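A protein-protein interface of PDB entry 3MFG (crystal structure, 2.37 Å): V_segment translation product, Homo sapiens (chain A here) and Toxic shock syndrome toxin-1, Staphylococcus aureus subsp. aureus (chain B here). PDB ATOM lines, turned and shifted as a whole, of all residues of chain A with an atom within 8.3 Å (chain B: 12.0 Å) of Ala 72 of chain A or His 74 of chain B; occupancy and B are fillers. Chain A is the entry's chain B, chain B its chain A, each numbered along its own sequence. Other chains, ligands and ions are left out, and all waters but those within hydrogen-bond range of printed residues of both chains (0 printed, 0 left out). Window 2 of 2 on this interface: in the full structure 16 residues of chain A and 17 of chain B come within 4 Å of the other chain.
NH1 of Arg 68 of chain B sits at hydrogen-bond distance from O of Gly 53 of chain A, 2.5 Å away.
The side-chain carboxylate (OE1) of Glu 52 of chain A lies within salt-bridge range of the side-chain amino group (NZ) of Lys 71 of chain B, 2.9 Å away.
The backbone NH (N) of Ser 72 of chain B is in hydrogen-bond range of the backbone carbonyl oxygen (O) of Gly 53 of chain A.
The backbone carbonyl oxygen of Ala 72 of chain A sits at hydrogen-bond distance from a ring nitrogen (NE2) of His 74 of chain B (3.0 Å).
OD2 of Asp 18 of chain B lies within salt-bridge range of NE of Arg 68 of chain B (2.8 Å).
The backbone carbonyl oxygen (O) of Tyr 80 of chain B lies within hydrogen-bond range of the backbone NH (N) of Ile 42 of chain B.
The guanidinium group (NH1) of Arg 68 of chain B lies within hydrogen-bond range of the side-chain hydroxyl (OG) of Ser 72 of chain B, 3.2 Å away.
The side-chain hydroxyl (OG) of Ser 72 of chain B is in hydrogen-bond range of a ring nitrogen (ND1) of His 82 of chain B, at 2.6 Å.
N of Glu 52 of chain A lies close to ND1 of His 71 of chain A (3.4 Å).
The backbone NH of Gly 53 of chain A lies within hydrogen-bond range of the backbone carbonyl oxygen of His 71 of chain A (3.3 Å).
Among the printed residues, merely in contact across the chains: Gly 53 of chain A with Lys 71 of chain B (3.99 Å), Gly 53 of chain A with Tyr 80 of chain B (3.6 Å) and Ser 54 of chain A with Arg 68 of chain B (3.95 Å).
Glu 52 of chain A touches just one residue of chain B: Lys 71.
No residue of chain B comes within 4 Å of His 71 of chain A.
Ala 72 of chain A touches one residue of chain B.
No residue of chain B comes within 4 Å of Ser 73 of chain A.
No residue of chain B comes within 4 Å of Leu 74 of chain A.
No residue of chain B comes within 4 Å of Leu 76 of chain A.
No residue of chain B comes within 4 Å of Ser 77 of chain A.
Asp 39 of chain B touches none of the printed residues of chain A.
Ile 42 of chain B touches none of the printed residues of chain A.
Printed residues of chain A within 4 Å of Lys 71 of chain B: Glu 52 (2.9 Å) and Gly 53 (3.99 Å).
Printed residues of chain A within 4 Å of Ser 72 of chain B: Gly 53.
His 74 of chain B touches just one residue of chain A: Ala 72.
The nearest residue of chain B that does not touch Ala 72 of chain A is Tyr 80 of chain B (4.02 Å).
The nearest printed residue of chain A that does not touch Tyr 80 of chain B is Ala 72 of chain A (4.02 Å).
Hydrophobic or aromatic side chains of chain B within 4 Å of the printed part of chain A: His 74 and Tyr 80.
Along chain B the printed residues that touch a printed residue of chain A span positions 68 to 80.
Of the 15 printed residues of chain A, 4 touch a printed residue of chain B.
Printed residues of chain A that touch a printed residue of chain B: Glu 52, Gly 53, Ser 54 and Ala 72.
Among the printed residues, 7 pairs touch across the chains.
Among the printed residues, Asp or Glu carboxylates within 4 Å of a Lys or Arg side-chain nitrogen of the other chain: Glu 52 of chain A with Lys 71 of chain B.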
ATOM      1  N   SER A  50      -2.963  27.775  36.576  1.00  0.00           N
ATOM      2  CA  SER A  50      -3.167  27.073  35.315  1.00  0.00           C
ATOM      3  C   SER A  50      -2.150  25.960  35.073  1.00  0.00           C
ATOM      4  O   SER A  50      -0.957  26.260  35.034  1.00  0.00           O
ATOM      5  CB  SER A  50      -3.058  28.088  34.197  1.00  0.00           C
ATOM      6  OG  SER A  50      -3.143  27.519  32.905  1.00  0.00           O
ATOM      7  N   ASN A  51      -2.608  24.698  34.969  1.00  0.00           N
ATOM      8  CA  ASN A  51      -1.752  23.598  34.507  1.00  0.00           C
ATOM      9  C   ASN A  51      -2.057  23.206  33.092  1.00  0.00           C
ATOM     10  O   ASN A  51      -3.209  23.251  32.641  1.00  0.00           O
ATOM     11  CB  ASN A  51      -1.856  22.345  35.378  1.00  0.00           C
ATOM     12  CG  ASN A  51      -1.368  22.588  36.804  1.00  0.00           C
ATOM     13  OD1 ASN A  51      -0.198  22.936  37.012  1.00  0.00           O
ATOM     14  ND2 ASN A  51      -2.271  22.475  37.766  1.00  0.00           N
ATOM     15  N   GLU A  52      -0.982  22.854  32.408  1.00  0.00           N
ATOM     16  CA  GLU A  52      -0.959  22.372  31.067  1.00  0.00           C
ATOM     17  C   GLU A  52      -2.031  21.282  30.891  1.00  0.00           C
ATOM     18  O   GLU A  52      -2.038  20.313  31.614  1.00  0.00           O
ATOM     19  CB  GLU A  52       0.428  21.785  30.798  1.00  0.00           C
ATOM     20  CG  GLU A  52       0.855  21.697  29.334  1.00  0.00           C
ATOM     21  CD  GLU A  52       0.183  20.589  28.581  1.00  0.00           C
ATOM     22  OE1 GLU A  52       0.070  19.478  29.163  1.00  0.00           O
ATOM     23  OE2 GLU A  52      -0.239  20.827  27.408  1.00  0.00           O
ATOM     24  N   GLY A  53      -2.990  21.520  29.999  1.00  0.00           N
ATOM     25  CA  GLY A  53      -3.937  20.452  29.642  1.00  0.00           C
ATOM     26  C   GLY A  53      -5.259  20.572  30.341  1.00  0.00           C
ATOM     27  O   GLY A  53      -6.242  20.125  29.809  1.00  0.00           O
ATOM     28  N   SER A  54      -5.280  21.245  31.499  1.00  0.00           N
ATOM     29  CA  SER A  54      -6.462  21.470  32.255  1.00  0.00           C
ATOM     30  C   SER A  54      -6.917  22.898  32.077  1.00  0.00           C
ATOM     31  O   SER A  54      -6.173  23.744  31.561  1.00  0.00           O
ATOM     32  CB  SER A  54      -6.132  21.247  33.717  1.00  0.00           C
ATOM     33  OG  SER A  54      -5.420  20.035  33.876  1.00  0.00           O
ATOM     34  N   ILE A  69      -7.931  31.561  29.713  1.00  0.00           N
ATOM     35  CA  ILE A  69      -6.557  31.157  29.827  1.00  0.00           C
ATOM     36  C   ILE A  69      -6.394  29.965  28.967  1.00  0.00           C
ATOM     37  O   ILE A  69      -7.175  29.039  29.066  1.00  0.00           O
ATOM     38  CB  ILE A  69      -6.179  30.861  31.290  1.00  0.00           C
ATOM     39  CG1 ILE A  69      -6.076  32.185  32.064  1.00  0.00           C
ATOM     40  CG2 ILE A  69      -4.845  30.149  31.388  1.00  0.00           C
ATOM     41  CD1 ILE A  69      -5.990  32.087  33.570  1.00  0.00           C
ATOM     42  N   ASN A  70      -5.357  29.963  28.143  1.00  0.00           N
ATOM     43  CA  ASN A  70      -4.977  28.835  27.303  1.00  0.00           C
ATOM     44  C   ASN A  70      -3.576  28.353  27.714  1.00  0.00           C
ATOM     45  O   ASN A  70      -2.704  29.134  28.015  1.00  0.00           O
ATOM     46  CB  ASN A  70      -4.983  29.284  25.839  1.00  0.00           C
ATOM     47  CG  ASN A  70      -6.351  29.182  25.212  1.00  0.00           C
ATOM     48  OD1 ASN A  70      -6.721  28.091  24.714  1.00  0.00           O
ATOM     49  ND2 ASN A  70      -7.144  30.255  25.280  1.00  0.00           N
ATOM     50  N   HIS A  71      -3.325  27.060  27.715  1.00  0.00           N
ATOM     51  CA  HIS A  71      -2.091  26.587  28.292  1.00  0.00           C
ATOM     52  C   HIS A  71      -1.834  25.198  27.765  1.00  0.00           C
ATOM     53  O   HIS A  71      -1.883  24.217  28.504  1.00  0.00           O
ATOM     54  CB  HIS A  71      -2.219  26.659  29.820  1.00  0.00           C
ATOM     55  CG  HIS A  71      -0.964  26.345  30.554  1.00  0.00           C
ATOM     56  ND1 HIS A  71      -0.921  26.219  31.924  1.00  0.00           N
ATOM     57  CD2 HIS A  71       0.283  26.084  30.109  1.00  0.00           C
ATOM     58  CE1 HIS A  71       0.307  25.876  32.286  1.00  0.00           C
ATOM     59  NE2 HIS A  71       1.052  25.775  31.199  1.00  0.00           N
ATOM     60  N   ALA A  72      -1.494  25.167  26.475  1.00  0.00           N
ATOM     61  CA  ALA A  72      -1.377  23.944  25.639  1.00  0.00           C
ATOM     62  C   ALA A  72       0.037  23.384  25.522  1.00  0.00           C
ATOM     63  O   ALA A  72       0.221  22.309  24.936  1.00  0.00           O
ATOM     64  CB  ALA A  72      -1.880  24.223  24.228  1.00  0.00           C
ATOM     65  N   SER A  73       1.048  24.103  25.987  1.00  0.00           N
ATOM     66  CA  SER A  73       2.393  23.526  26.039  1.00  0.00           C
ATOM     67  C   SER A  73       3.019  23.842  27.371  1.00  0.00           C
ATOM     68  O   SER A  73       2.498  24.649  28.119  1.00  0.00           O
ATOM     69  CB  SER A  73       3.256  24.089  24.933  1.00  0.00           C
ATOM     70  OG  SER A  73       3.549  25.429  25.208  1.00  0.00           O
ATOM     71  N   LEU A  74       4.127  23.205  27.682  1.00  0.00           N
ATOM     72  CA  LEU A  74       4.799  23.413  28.970  1.00  0.00           C
ATOM     73  C   LEU A  74       5.576  24.761  29.053  1.00  0.00           C
ATOM     74  O   LEU A  74       6.169  25.104  30.063  1.00  0.00           O
ATOM     75  CB  LEU A  74       5.731  22.227  29.222  1.00  0.00           C
ATOM     76  CG  LEU A  74       4.974  20.910  29.523  1.00  0.00           C
ATOM     77  CD1 LEU A  74       5.969  19.742  29.506  1.00  0.00           C
ATOM     78  CD2 LEU A  74       4.166  21.021  30.881  1.00  0.00           C
ATOM     79  N   THR A  75       5.495  25.528  27.988  1.00  0.00           N
ATOM     80  CA  THR A  75       6.308  26.690  27.762  1.00  0.00           C
ATOM     81  C   THR A  75       5.503  27.982  27.669  1.00  0.00           C
ATOM     82  O   THR A  75       6.069  29.060  27.831  1.00  0.00           O
ATOM     83  CB  THR A  75       7.045  26.497  26.429  1.00  0.00           C
ATOM     84  OG1 THR A  75       8.215  25.717  26.695  1.00  0.00           O
ATOM     85  CG2 THR A  75       7.400  27.843  25.768  1.00  0.00           C
ATOM     86  N   LEU A  76       4.201  27.881  27.413  1.00  0.00           N
ATOM     87  CA  LEU A  76       3.387  29.068  27.124  1.00  0.00           C
ATOM     88  C   LEU A  76       2.037  29.018  27.807  1.00  0.00           C
ATOM     89  O   LEU A  76       1.393  27.963  27.826  1.00  0.00           O
ATOM     90  CB  LEU A  76       3.156  29.172  25.602  1.00  0.00           C
ATOM     91  CG  LEU A  76       2.138  30.190  25.088  1.00  0.00           C
ATOM     92  CD1 LEU A  76       2.522  31.600  25.529  1.00  0.00           C
ATOM     93  CD2 LEU A  76       1.925  30.099  23.507  1.00  0.00           C
ATOM     94  N   SER A  77       1.575  30.157  28.280  1.00  0.00           N
ATOM     95  CA  SER A  77       0.177  30.311  28.668  1.00  0.00           C
ATOM     96  C   SER A  77      -0.287  31.679  28.206  1.00  0.00           C
ATOM     97  O   SER A  77       0.497  32.601  28.245  1.00  0.00           O
ATOM     98  CB  SER A  77       0.077  30.208  30.179  1.00  0.00           C
ATOM     99  OG  SER A  77      -1.025  30.914  30.668  1.00  0.00           O
ATOM    100  N   THR A  78      -1.550  31.838  27.829  1.00  0.00           N
ATOM    101  CA  THR A  78      -2.084  33.114  27.234  1.00  0.00           C
ATOM    102  C   THR A  78      -3.301  33.502  27.986  1.00  0.00           C
ATOM    103  O   THR A  78      -4.203  32.669  28.164  1.00  0.00           O
ATOM    104  CB  THR A  78      -2.465  32.924  25.763  1.00  0.00           C
ATOM    105  OG1 THR A  78      -1.301  32.488  25.033  1.00  0.00           O
ATOM    106  CG2 THR A  78      -3.026  34.187  25.133  1.00  0.00           C
ATOM    107  N   ASP B  18     -14.797  24.713  28.364  1.00  0.00           N
ATOM    108  CA  ASP B  18     -14.459  24.840  26.970  1.00  0.00           C
ATOM    109  C   ASP B  18     -15.687  25.224  26.260  1.00  0.00           C
ATOM    110  O   ASP B  18     -16.705  24.535  26.407  1.00  0.00           O
ATOM    111  CB  ASP B  18     -13.972  23.526  26.406  1.00  0.00           C
ATOM    112  CG  ASP B  18     -12.682  23.113  26.932  1.00  0.00           C
ATOM    113  OD1 ASP B  18     -11.784  23.975  27.037  1.00  0.00           O
ATOM    114  OD2 ASP B  18     -12.515  21.900  27.195  1.00  0.00           O
ATOM    115  N   PHE B  20     -16.799  25.825  22.453  1.00  0.00           N
ATOM    116  CA  PHE B  20     -16.439  25.768  21.028  1.00  0.00           C
ATOM    117  C   PHE B  20     -17.646  26.041  20.163  1.00  0.00           C
ATOM    118  O   PHE B  20     -18.739  25.663  20.547  1.00  0.00           O
ATOM    119  CB  PHE B  20     -15.893  24.413  20.698  1.00  0.00           C
ATOM    120  CG  PHE B  20     -14.536  24.152  21.235  1.00  0.00           C
ATOM    121  CD1 PHE B  20     -13.424  24.616  20.574  1.00  0.00           C
ATOM    122  CD2 PHE B  20     -14.348  23.364  22.365  1.00  0.00           C
ATOM    123  CE1 PHE B  20     -12.131  24.329  21.060  1.00  0.00           C
ATOM    124  CE2 PHE B  20     -13.069  23.084  22.838  1.00  0.00           C
ATOM    125  CZ  PHE B  20     -11.982  23.592  22.206  1.00  0.00           C
ATOM    126  N   ASP B  39     -10.319  24.656  15.718  1.00  0.00           N
ATOM    127  CA  ASP B  39      -8.893  24.922  15.929  1.00  0.00           C
ATOM    128  C   ASP B  39      -8.108  23.669  15.725  1.00  0.00           C
ATOM    129  O   ASP B  39      -6.953  23.607  16.091  1.00  0.00           O
ATOM    130  CB  ASP B  39      -8.606  25.441  17.358  1.00  0.00           C
ATOM    131  CG  ASP B  39      -8.980  24.389  18.495  1.00  0.00           C
ATOM    132  OD1 ASP B  39      -9.595  23.316  18.154  1.00  0.00           O
ATOM    133  OD2 ASP B  39      -8.652  24.662  19.714  1.00  0.00           O
ATOM    134  N   GLY B  40      -8.768  22.627  15.248  1.00  0.00           N
ATOM    135  CA  GLY B  40      -8.091  21.356  14.923  1.00  0.00           C
ATOM    136  C   GLY B  40      -7.941  20.414  16.113  1.00  0.00           C
ATOM    137  O   GLY B  40      -7.383  19.310  15.979  1.00  0.00           O
ATOM    138  N   SER B  41      -8.397  20.839  17.291  1.00  0.00           N
ATOM    139  CA  SER B  41      -8.461  19.899  18.442  1.00  0.00           C
ATOM    140  C   SER B  41      -9.571  18.846  18.171  1.00  0.00           C
ATOM    141  O   SER B  41     -10.579  19.075  17.455  1.00  0.00           O
ATOM    142  CB  SER B  41      -8.666  20.648  19.818  1.00  0.00           C
ATOM    143  OG  SER B  41      -9.954  21.306  19.950  1.00  0.00           O
ATOM    144  N   ILE B  42      -9.371  17.683  18.753  1.00  0.00           N
ATOM    145  CA  ILE B  42     -10.377  16.649  18.749  1.00  0.00           C
ATOM    146  C   ILE B  42     -10.972  16.479  20.129  1.00  0.00           C
ATOM    147  O   ILE B  42     -10.239  16.302  21.069  1.00  0.00           O
ATOM    148  CB  ILE B  42      -9.760  15.288  18.367  1.00  0.00           C
ATOM    149  CG1 ILE B  42      -9.358  15.288  16.885  1.00  0.00           C
ATOM    150  CG2 ILE B  42     -10.797  14.185  18.543  1.00  0.00           C
ATOM    151  CD1 ILE B  42      -8.863  13.865  16.425  1.00  0.00           C
ATOM    152  N   SER B  43     -12.303  16.470  20.220  1.00  0.00           N
ATOM    153  CA  SER B  43     -13.014  16.253  21.475  1.00  0.00           C
ATOM    154  C   SER B  43     -13.638  14.871  21.544  1.00  0.00           C
ATOM    155  O   SER B  43     -14.460  14.537  20.696  1.00  0.00           O
ATOM    156  CB  SER B  43     -14.137  17.275  21.585  1.00  0.00           C
ATOM    157  OG  SER B  43     -13.648  18.543  21.997  1.00  0.00           O
ATOM    158  N   LEU B  44     -13.229  14.082  22.537  1.00  0.00           N
ATOM    159  CA  LEU B  44     -13.876  12.838  22.896  1.00  0.00           C
ATOM    160  C   LEU B  44     -14.837  13.128  24.095  1.00  0.00           C
ATOM    161  O   LEU B  44     -14.412  13.248  25.231  1.00  0.00           O
ATOM    162  CB  LEU B  44     -12.810  11.792  23.262  1.00  0.00           C
ATOM    163  CG  LEU B  44     -11.770  11.546  22.149  1.00  0.00           C
ATOM    164  CD1 LEU B  44     -10.693  10.416  22.399  1.00  0.00           C
ATOM    165  CD2 LEU B  44     -12.479  11.292  20.793  1.00  0.00           C
ATOM    166  N   ARG B  68     -13.958  19.314  31.215  1.00  0.00           N
ATOM    167  CA  ARG B  68     -12.997  18.331  30.992  1.00  0.00           C
ATOM    168  C   ARG B  68     -12.991  17.382  32.130  1.00  0.00           C
ATOM    169  O   ARG B  68     -13.011  17.801  33.239  1.00  0.00           O
ATOM    170  CB  ARG B  68     -11.590  18.962  30.860  1.00  0.00           C
ATOM    171  CG  ARG B  68     -11.507  19.986  29.820  1.00  0.00           C
ATOM    172  CD  ARG B  68     -10.031  20.298  29.447  1.00  0.00           C
ATOM    173  NE  ARG B  68     -10.045  21.343  28.435  1.00  0.00           N
ATOM    174  CZ  ARG B  68      -8.931  21.959  27.979  1.00  0.00           C
ATOM    175  NH1 ARG B  68      -7.725  21.635  28.420  1.00  0.00           N
ATOM    176  NH2 ARG B  68      -9.026  22.947  27.104  1.00  0.00           N
ATOM    177  N   LYS B  70     -10.567  14.894  32.417  1.00  0.00           N
ATOM    178  CA  LYS B  70      -9.170  14.770  32.776  1.00  0.00           C
ATOM    179  C   LYS B  70      -8.290  15.624  31.795  1.00  0.00           C
ATOM    180  O   LYS B  70      -8.755  16.253  30.853  1.00  0.00           O
ATOM    181  CB  LYS B  70      -8.756  13.284  32.793  1.00  0.00           C
ATOM    182  CG  LYS B  70      -8.936  12.634  31.415  1.00  0.00           C
ATOM    183  CD  LYS B  70      -8.561  11.173  31.334  1.00  0.00           C
ATOM    184  CE  LYS B  70      -8.474  10.747  29.894  1.00  0.00           C
ATOM    185  NZ  LYS B  70      -8.489   9.282  29.711  1.00  0.00           N
ATOM    186  N   LYS B  71      -7.005  15.594  32.038  1.00  0.00           N
ATOM    187  CA  LYS B  71      -6.051  16.438  31.356  1.00  0.00           C
ATOM    188  C   LYS B  71      -6.073  16.138  29.863  1.00  0.00           C
ATOM    189  O   LYS B  71      -6.020  14.965  29.468  1.00  0.00           O
ATOM    190  CB  LYS B  71      -4.695  16.161  31.989  1.00  0.00           C
ATOM    191  CG  LYS B  71      -3.444  16.829  31.399  1.00  0.00           C
ATOM    192  CD  LYS B  71      -2.271  16.774  32.450  1.00  0.00           C
ATOM    193  CE  LYS B  71      -0.881  16.487  31.819  1.00  0.00           C
ATOM    194  NZ  LYS B  71      -0.787  16.974  30.421  1.00  0.00           N
ATOM    195  N   SER B  72      -6.281  17.194  29.061  1.00  0.00           N
ATOM    196  CA  SER B  72      -6.106  17.132  27.638  1.00  0.00           C
ATOM    197  C   SER B  72      -4.651  16.658  27.257  1.00  0.00           C
ATOM    198  O   SER B  72      -3.686  16.908  27.970  1.00  0.00           O
ATOM    199  CB  SER B  72      -6.453  18.462  26.995  1.00  0.00           C
ATOM    200  OG  SER B  72      -7.824  18.779  27.087  1.00  0.00           O
ATOM    201  N   GLN B  73      -4.528  15.950  26.135  1.00  0.00           N
ATOM    202  CA  GLN B  73      -3.275  15.294  25.756  1.00  0.00           C
ATOM    203  C   GLN B  73      -2.987  15.491  24.289  1.00  0.00           C
ATOM    204  O   GLN B  73      -3.877  15.774  23.518  1.00  0.00           O
ATOM    205  CB  GLN B  73      -3.326  13.792  26.081  1.00  0.00           C
ATOM    206  CG  GLN B  73      -3.113  13.429  27.582  1.00  0.00           C
ATOM    207  CD  GLN B  73      -1.670  13.647  28.100  1.00  0.00           C
ATOM    208  OE1 GLN B  73      -0.739  14.001  27.342  1.00  0.00           O
ATOM    209  NE2 GLN B  73      -1.485  13.435  29.401  1.00  0.00           N
ATOM    210  N   HIS B  74      -1.713  15.382  23.924  1.00  0.00           N
ATOM    211  CA  HIS B  74      -1.273  15.488  22.524  1.00  0.00           C
ATOM    212  C   HIS B  74      -0.872  14.092  22.060  1.00  0.00           C
ATOM    213  O   HIS B  74      -0.350  13.298  22.831  1.00  0.00           O
ATOM    214  CB  HIS B  74      -0.070  16.435  22.383  1.00  0.00           C
ATOM    215  CG  HIS B  74      -0.382  17.897  22.599  1.00  0.00           C
ATOM    216  ND1 HIS B  74      -0.769  18.739  21.575  1.00  0.00           N
ATOM    217  CD2 HIS B  74      -0.337  18.667  23.717  1.00  0.00           C
ATOM    218  CE1 HIS B  74      -0.934  19.965  22.049  1.00  0.00           C
ATOM    219  NE2 HIS B  74      -0.686  19.946  23.345  1.00  0.00           N
ATOM    220  N   THR B  75      -1.136  13.774  20.800  1.00  0.00           N
ATOM    221  CA  THR B  75      -0.741  12.458  20.251  1.00  0.00           C
ATOM    222  C   THR B  75       0.649  12.603  19.631  1.00  0.00           C
ATOM    223  O   THR B  75       1.511  13.309  20.153  1.00  0.00           O
ATOM    224  CB  THR B  75      -1.762  11.968  19.169  1.00  0.00           C
ATOM    225  OG1 THR B  75      -1.849  12.933  18.123  1.00  0.00           O
ATOM    226  CG2 THR B  75      -3.133  11.773  19.764  1.00  0.00           C
ATOM    227  N   SER B  76       0.855  11.888  18.529  1.00  0.00           N
ATOM    228  CA  SER B  76       1.795  12.275  17.476  1.00  0.00           C
ATOM    229  C   SER B  76       1.270  11.599  16.199  1.00  0.00           C
ATOM    230  O   SER B  76       1.109  10.363  16.224  1.00  0.00           O
ATOM    231  CB  SER B  76       3.194  11.810  17.847  1.00  0.00           C
ATOM    232  OG  SER B  76       3.128  10.452  18.274  1.00  0.00           O
ATOM    233  N   GLU B  77       0.961  12.308  15.096  1.00  0.00           N
ATOM    234  CA  GLU B  77       1.281  13.722  14.812  1.00  0.00           C
ATOM    235  C   GLU B  77       1.663  14.557  16.016  1.00  0.00           C
ATOM    236  O   GLU B  77       2.729  14.349  16.618  1.00  0.00           O
ATOM    237  CB  GLU B  77       0.110  14.385  14.048  1.00  0.00           C
ATOM    238  N   GLY B  78       0.848  15.556  16.309  1.00  0.00           N
ATOM    239  CA  GLY B  78       0.708  16.087  17.670  1.00  0.00           C
ATOM    240  C   GLY B  78      -0.732  16.617  17.748  1.00  0.00           C
ATOM    241  O   GLY B  78      -0.959  17.830  17.895  1.00  0.00           O
ATOM    242  N   THR B  79      -1.721  15.732  17.579  1.00  0.00           N
ATOM    243  CA  THR B  79      -3.100  16.215  17.611  1.00  0.00           C
ATOM    244  C   THR B  79      -3.447  16.435  19.067  1.00  0.00           C
ATOM    245  O   THR B  79      -2.986  15.699  19.924  1.00  0.00           O
ATOM    246  CB  THR B  79      -4.102  15.290  16.886  1.00  0.00           C
ATOM    247  OG1 THR B  79      -3.522  14.865  15.645  1.00  0.00           O
ATOM    248  CG2 THR B  79      -5.413  16.061  16.595  1.00  0.00           C
ATOM    249  N   TYR B  80      -4.163  17.517  19.329  1.00  0.00           N
ATOM    250  CA  TYR B  80      -4.583  17.862  20.682  1.00  0.00           C
ATOM    251  C   TYR B  80      -5.955  17.259  20.973  1.00  0.00           C
ATOM    252  O   TYR B  80      -6.917  17.574  20.307  1.00  0.00           O
ATOM    253  CB  TYR B  80      -4.637  19.387  20.844  1.00  0.00           C
ATOM    254  CG  TYR B  80      -4.608  19.890  22.279  1.00  0.00           C
ATOM    255  CD1 TYR B  80      -3.968  19.186  23.274  1.00  0.00           C
ATOM    256  CD2 TYR B  80      -5.159  21.119  22.612  1.00  0.00           C
ATOM    257  CE1 TYR B  80      -3.901  19.665  24.578  1.00  0.00           C
ATOM    258  CE2 TYR B  80      -5.063  21.646  23.928  1.00  0.00           C
ATOM    259  CZ  TYR B  80      -4.472  20.888  24.904  1.00  0.00           C
ATOM    260  OH  TYR B  80      -4.385  21.336  26.224  1.00  0.00           O
ATOM    261  N   ILE B  81      -6.038  16.391  21.964  1.00  0.00           N
ATOM    262  CA  ILE B  81      -7.362  15.749  22.327  1.00  0.00           C
ATOM    263  C   ILE B  81      -7.895  16.189  23.662  1.00  0.00           C
ATOM    264  O   ILE B  81      -7.201  16.128  24.675  1.00  0.00           O
ATOM    265  CB  ILE B  81      -7.279  14.215  22.405  1.00  0.00           C
ATOM    266  CG1 ILE B  81      -6.598  13.644  21.163  1.00  0.00           C
ATOM    267  CG2 ILE B  81      -8.695  13.598  22.473  1.00  0.00           C
ATOM    268  CD1 ILE B  81      -5.870  12.409  21.541  1.00  0.00           C
ATOM    269  N   HIS B  82      -9.144  16.609  23.652  1.00  0.00           N
ATOM    270  CA  HIS B  82      -9.880  17.006  24.826  1.00  0.00           C
ATOM    271  C   HIS B  82     -10.829  15.849  25.216  1.00  0.00           C
ATOM    272  O   HIS B  82     -11.514  15.269  24.337  1.00  0.00           O
ATOM    273  CB  HIS B  82     -10.687  18.237  24.476  1.00  0.00           C
ATOM    274  CG  HIS B  82      -9.858  19.427  24.144  1.00  0.00           C
ATOM    275  ND1 HIS B  82      -8.837  19.866  24.963  1.00  0.00           N
ATOM    276  CD2 HIS B  82      -9.903  20.289  23.091  1.00  0.00           C
ATOM    277  CE1 HIS B  82      -8.271  20.922  24.409  1.00  0.00           C
ATOM    278  NE2 HIS B  82      -8.903  21.206  23.280  1.00  0.00           N
ATOM    279  N   PHE B  83     -10.829  15.484  26.500  1.00  0.00           N
ATOM    280  CA  PHE B  83     -11.752  14.502  27.117  1.00  0.00           C
ATOM    281  C   PHE B  83     -12.745  15.209  27.953  1.00  0.00           C
ATOM    282  O   PHE B  83     -12.382  15.810  28.979  1.00  0.00           O
ATOM    283  CB  PHE B  83     -10.978  13.646  28.066  1.00  0.00           C
ATOM    284  CG  PHE B  83      -9.851  12.934  27.404  1.00  0.00           C
ATOM    285  CD1 PHE B  83     -10.076  11.721  26.730  1.00  0.00           C
ATOM    286  CD2 PHE B  83      -8.571  13.483  27.411  1.00  0.00           C
ATOM    287  CE1 PHE B  83      -9.017  11.064  26.095  1.00  0.00           C
ATOM    288  CE2 PHE B  83      -7.511  12.842  26.776  1.00  0.00           C
ATOM    289  CZ  PHE B  83      -7.717  11.642  26.091  1.00  0.00           C
